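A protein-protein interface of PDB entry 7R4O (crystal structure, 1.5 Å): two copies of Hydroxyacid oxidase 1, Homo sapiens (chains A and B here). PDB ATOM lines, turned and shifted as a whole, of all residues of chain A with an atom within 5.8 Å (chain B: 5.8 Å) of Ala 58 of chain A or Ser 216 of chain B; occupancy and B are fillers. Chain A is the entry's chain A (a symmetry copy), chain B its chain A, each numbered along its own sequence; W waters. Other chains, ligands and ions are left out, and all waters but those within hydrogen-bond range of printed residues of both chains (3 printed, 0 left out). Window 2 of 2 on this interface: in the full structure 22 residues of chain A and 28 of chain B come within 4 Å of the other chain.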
ATOM      1  N   ARG A  55      20.557  10.366  16.311  1.00  0.00           N
ATOM      2  CA  ARG A  55      20.098  10.746  14.948  1.00  0.00           C
ATOM      3  C   ARG A  55      19.154  11.951  14.952  1.00  0.00           C
ATOM      4  O   ARG A  55      18.835  12.393  13.863  1.00  0.00           O
ATOM      5  CB  ARG A  55      19.351   9.584  14.296  1.00  0.00           C
ATOM      6  CG  ARG A  55      20.188   8.325  14.137  1.00  0.00           C
ATOM      7  CD  ARG A  55      20.734   8.266  12.731  1.00  0.00           C
ATOM      8  NE  ARG A  55      22.163   8.491  12.780  1.00  0.00           N
ATOM      9  CZ  ARG A  55      22.978   8.371  11.746  1.00  0.00           C
ATOM     10  NH1 ARG A  55      22.497   8.019  10.565  1.00  0.00           N
ATOM     11  NH2 ARG A  55      24.267   8.596  11.902  1.00  0.00           N
ATOM     12  N   ASN A  56      18.742  12.453  16.100  1.00  0.00           N
ATOM     13  CA  ASN A  56      17.754  13.570  16.216  1.00  0.00           C
ATOM     14  C   ASN A  56      16.345  13.050  15.930  1.00  0.00           C
ATOM     15  O   ASN A  56      15.933  13.083  14.814  1.00  0.00           O
ATOM     16  CB  ASN A  56      18.023  14.820  15.380  1.00  0.00           C
ATOM     17  CG  ASN A  56      17.053  15.932  15.716  1.00  0.00           C
ATOM     18  OD1 ASN A  56      16.107  15.734  16.467  1.00  0.00           O
ATOM     19  ND2 ASN A  56      17.287  17.112  15.171  1.00  0.00           N
ATOM     20  N   VAL A  57      15.656  12.655  16.998  1.00  0.00           N
ATOM     21  CA  VAL A  57      14.295  12.082  16.862  1.00  0.00           C
ATOM     22  C   VAL A  57      13.312  12.908  17.674  1.00  0.00           C
ATOM     23  O   VAL A  57      12.289  12.358  18.175  1.00  0.00           O
ATOM     24  CB  VAL A  57      14.306  10.596  17.267  1.00  0.00           C
ATOM     25  CG1 VAL A  57      15.033   9.756  16.253  1.00  0.00           C
ATOM     26  CG2 VAL A  57      14.837  10.339  18.651  1.00  0.00           C
ATOM     27  N   ALA A  58      13.537  14.223  17.767  1.00  0.00           N
ATOM     28  CA  ALA A  58      12.625  15.143  18.470  1.00  0.00           C
ATOM     29  C   ALA A  58      11.317  15.214  17.694  1.00  0.00           C
ATOM     30  O   ALA A  58      10.244  15.431  18.322  1.00  0.00           O
ATOM     31  CB  ALA A  58      13.264  16.515  18.547  1.00  0.00           C
ATOM     32  N   GLU A  59      11.415  15.087  16.386  1.00  0.00           N
ATOM     33  CA  GLU A  59      10.284  15.281  15.471  1.00  0.00           C
ATOM     34  C   GLU A  59      10.188  13.876  14.935  1.00  0.00           C
ATOM     35  O   GLU A  59      11.212  13.418  14.369  1.00  0.00           O
ATOM     36  CB  GLU A  59      10.548  16.380  14.436  1.00  0.00           C
ATOM     37  N   THR A  60       9.199  13.122  15.371  1.00  0.00           N
ATOM     38  CA  THR A  60       8.961  11.793  14.732  1.00  0.00           C
ATOM     39  C   THR A  60       7.691  11.949  13.897  1.00  0.00           C
ATOM     40  O   THR A  60       6.693  12.459  14.432  1.00  0.00           O
ATOM     41  CB  THR A  60       8.969  10.627  15.741  1.00  0.00           C
ATOM     42  OG1 THR A  60      10.222  10.570  16.432  1.00  0.00           O
ATOM     43  CG2 THR A  60       8.866   9.243  15.131  1.00  0.00           C
ATOM     44  N   ARG B 137      21.312  22.640  28.665  1.00  0.00           N
ATOM     45  CA  ARG B 137      22.766  22.435  28.465  1.00  0.00           C
ATOM     46  C   ARG B 137      23.513  23.095  29.620  1.00  0.00           C
ATOM     47  O   ARG B 137      24.616  22.650  29.884  1.00  0.00           O
ATOM     48  CB  ARG B 137      23.262  22.917  27.103  1.00  0.00           C
ATOM     49  CG  ARG B 137      22.611  22.188  25.945  1.00  0.00           C
ATOM     50  CD  ARG B 137      22.961  20.697  25.925  1.00  0.00           C
ATOM     51  NE  ARG B 137      22.761  20.229  24.561  1.00  0.00           N
ATOM     52  CZ  ARG B 137      21.576  19.842  24.093  1.00  0.00           C
ATOM     53  NH1 ARG B 137      20.542  19.804  24.909  1.00  0.00           N
ATOM     54  NH2 ARG B 137      21.488  19.484  22.836  1.00  0.00           N
ATOM     55  N   PRO B 162      16.848   8.808  23.900  1.00  0.00           N
ATOM     56  CA  PRO B 162      16.198  10.067  23.510  1.00  0.00           C
ATOM     57  C   PRO B 162      14.847  10.225  24.189  1.00  0.00           C
ATOM     58  O   PRO B 162      14.376  11.355  24.389  1.00  0.00           O
ATOM     59  CB  PRO B 162      16.066   9.974  22.018  1.00  0.00           C
ATOM     60  CG  PRO B 162      15.994   8.429  21.740  1.00  0.00           C
ATOM     61  CD  PRO B 162      16.936   7.865  22.787  1.00  0.00           C
ATOM     62  N   TYR B 163      14.189   9.107  24.414  1.00  0.00           N
ATOM     63  CA  TYR B 163      12.965   8.932  25.213  1.00  0.00           C
ATOM     64  C   TYR B 163      13.172   7.737  26.122  1.00  0.00           C
ATOM     65  O   TYR B 163      14.005   6.888  25.764  1.00  0.00           O
ATOM     66  CB  TYR B 163      11.738   8.718  24.313  1.00  0.00           C
ATOM     67  CG  TYR B 163      11.425   9.844  23.365  1.00  0.00           C
ATOM     68  CD1 TYR B 163      10.667  10.937  23.775  1.00  0.00           C
ATOM     69  CD2 TYR B 163      11.893   9.836  22.077  1.00  0.00           C
ATOM     70  CE1 TYR B 163      10.441  11.984  22.901  1.00  0.00           C
ATOM     71  CE2 TYR B 163      11.642  10.855  21.175  1.00  0.00           C
ATOM     72  CZ  TYR B 163      10.926  11.956  21.611  1.00  0.00           C
ATOM     73  OH  TYR B 163      10.739  12.933  20.650  1.00  0.00           O
ATOM     74  N   ASP B 214      16.808  15.383  26.266  1.00  0.00           N
ATOM     75  CA  ASP B 214      16.696  15.968  24.920  1.00  0.00           C
ATOM     76  C   ASP B 214      16.610  14.884  23.855  1.00  0.00           C
ATOM     77  O   ASP B 214      17.605  14.238  23.528  1.00  0.00           O
ATOM     78  CB  ASP B 214      17.843  16.929  24.677  1.00  0.00           C
ATOM     79  CG  ASP B 214      17.624  17.832  23.489  1.00  0.00           C
ATOM     80  OD1 ASP B 214      16.824  17.479  22.592  1.00  0.00           O
ATOM     81  OD2 ASP B 214      18.395  18.843  23.402  1.00  0.00           O
ATOM     82  N   PRO B 215      15.462  14.729  23.167  1.00  0.00           N
ATOM     83  CA  PRO B 215      15.387  13.724  22.107  1.00  0.00           C
ATOM     84  C   PRO B 215      16.057  14.143  20.809  1.00  0.00           C
ATOM     85  O   PRO B 215      16.179  13.372  19.917  1.00  0.00           O
ATOM     86  CB  PRO B 215      13.885  13.532  21.929  1.00  0.00           C
ATOM     87  CG  PRO B 215      13.342  14.927  22.226  1.00  0.00           C
ATOM     88  CD  PRO B 215      14.176  15.388  23.417  1.00  0.00           C
ATOM     89  N   SER B 216      16.506  15.406  20.721  1.00  0.00           N
ATOM     90  CA  SER B 216      17.200  15.948  19.546  1.00  0.00           C
ATOM     91  C   SER B 216      18.688  15.635  19.496  1.00  0.00           C
ATOM     92  O   SER B 216      19.298  16.003  18.471  1.00  0.00           O
ATOM     93  CB  SER B 216      16.957  17.440  19.391  1.00  0.00           C
ATOM     94  OG  SER B 216      17.766  18.172  20.291  1.00  0.00           O
ATOM     95  N   ILE B 217      19.249  14.987  20.496  1.00  0.00           N
ATOM     96  CA  ILE B 217      20.735  15.002  20.447  1.00  0.00           C
ATOM     97  C   ILE B 217      21.251  14.171  19.279  1.00  0.00           C
ATOM     98  O   ILE B 217      20.659  13.105  18.864  1.00  0.00           O
ATOM     99  CB  ILE B 217      21.370  14.615  21.769  1.00  0.00           C
ATOM    100  CG1 ILE B 217      20.950  13.228  22.221  1.00  0.00           C
ATOM    101  CG2 ILE B 217      21.080  15.705  22.811  1.00  0.00           C
ATOM    102  CD1 ILE B 217      21.968  12.624  23.198  1.00  0.00           C
ATOM    103  N   SER B 218      22.343  14.644  18.735  1.00  0.00           N
ATOM    104  CA  SER B 218      22.965  14.117  17.519  1.00  0.00           C
ATOM    105  C   SER B 218      24.457  14.043  17.787  1.00  0.00           C
ATOM    106  O   SER B 218      24.937  14.370  18.934  1.00  0.00           O
ATOM    107  CB  SER B 218      22.673  14.988  16.309  1.00  0.00           C
ATOM    108  OG  SER B 218      23.505  16.127  16.320  1.00  0.00           O
ATOM    109  N   ASP B 221      26.075  17.133  19.225  1.00  0.00           N
ATOM    110  CA  ASP B 221      26.077  17.272  20.699  1.00  0.00           C
ATOM    111  C   ASP B 221      27.276  16.510  21.288  1.00  0.00           C
ATOM    112  O   ASP B 221      27.786  16.911  22.319  1.00  0.00           O
ATOM    113  CB  ASP B 221      24.721  16.857  21.255  1.00  0.00           C
ATOM    114  CG  ASP B 221      23.673  17.792  20.703  1.00  0.00           C
ATOM    115  OD1 ASP B 221      23.749  18.976  21.054  1.00  0.00           O
ATOM    116  OD2 ASP B 221      22.858  17.367  19.840  1.00  0.00           O
HETATM  117  O   HOH W   1      18.471  11.739  19.337  1.00  0.00           O
HETATM  118  O   HOH W   2      20.208  17.954  16.726  1.00  0.00           O
HETATM  119  O   HOH W   3       8.655  11.991  18.990  1.00  0.00           O
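Of chain B, only Tyr 163 (3.5 Å), Pro 215 (3.5 Å) and Ser 216 (3.9 Å) come within 4 Å of Ala 58 of chain A.
Of the printed residues of chain A, Ser 216 of chain B touches Asn 56 (3.3 Å) and Ala 58 (3.9 Å).
Printed residues of chain B within 4 Å of Val 57 of chain A: Pro 162, Tyr 163 and Pro 215.
Of the printed residues of chain A, Pro 162 of chain B touches Val 57.
Of the printed residues of chain A, Ile 217 of chain B touches Arg 55 and Asn 56.
Ser 218 of chain B touches none of the printed residues of chain A.
Asp 221 of chain B touches none of the printed residues of chain A.
The nearest residue of chain A that does not touch Ser 216 of chain B is Val 57 of chain A (4.4 Å).
Printed residues of chain B that touch a printed residue of chain A: Pro 162, Tyr 163, Pro 215, Ser 216 and Ile 217.
Hydrophobic or aromatic side chains of chain B within 4 Å of the printed part of chain A: Pro 162, Tyr 163 and Pro 215.
Among the printed residues, 9 pairs touch across the chains.
Among the printed residues, no Asp or Glu carboxylate lies within 4 Å of a Lys or Arg side-chain nitrogen of the other chain.
The side-chain hydroxyl (OH) of Tyr 163 of chain B sits at hydrogen-bond distance from the backbone carbonyl oxygen (O) of Val 57 of chain A (3.0 Å).
The backbone carbonyl oxygen (O) of Ala 58 of chain A sits at hydrogen-bond distance from the side-chain hydroxyl (OH) of Tyr 163 of chain B (3.5 Å).
N of Val 57 of chain A sits at hydrogen-bond distance from O of Pro 215 of chain B (3.1 Å).
O of Ile 217 of chain B sits at hydrogen-bond distance from N of Asn 56 of chain A (3.4 Å).
No position is printed for both chains.
The side-chain carboxylate (OD1) of Asp 214 of chain B sits at hydrogen-bond distance from the side-chain hydroxyl (OG) of Ser 216 of chain B (2.6 Å).
OD1 of Asn 56 of chain A lies within hydrogen-bond range of N of Ala 58 of chain A (3.3 Å).
The side-chain hydroxyl of Thr 60 of chain A sits at hydrogen-bond distance from the backbone carbonyl oxygen of Val 57 of chain A, at 3.2 Å.
Among the printed residues, pairs that only touch across the chains: Arg 55 of chain A with Ile 217 of chain B, Asn 56 of chain A with Ser 216 of chain B, Val 57 of chain A with Pro 162 of chain B, Ala 58 of chain A with Pro 215 of chain B and Ala 58 of chain A with Ser 216 of chain B.
Water W1 lies within hydrogen-bond range of O of Ile 217 of chain B (2.6 Å), O of Pro 215 of chain B (2.9 Å) and N of Asn 56 of chain A (3.3 Å).
Water W2 lies within hydrogen-bond range of the backbone carbonyl oxygen (O) of Ser 216 of chain B (2.8 Å) and the side-chain amide nitrogen (ND2) of Asn 56 of chain A (3.4 Å).
Water W3 bridges the side-chain hydroxyl of Tyr 163 of chain B and the side-chain hydroxyl of Thr 60 of chain A.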
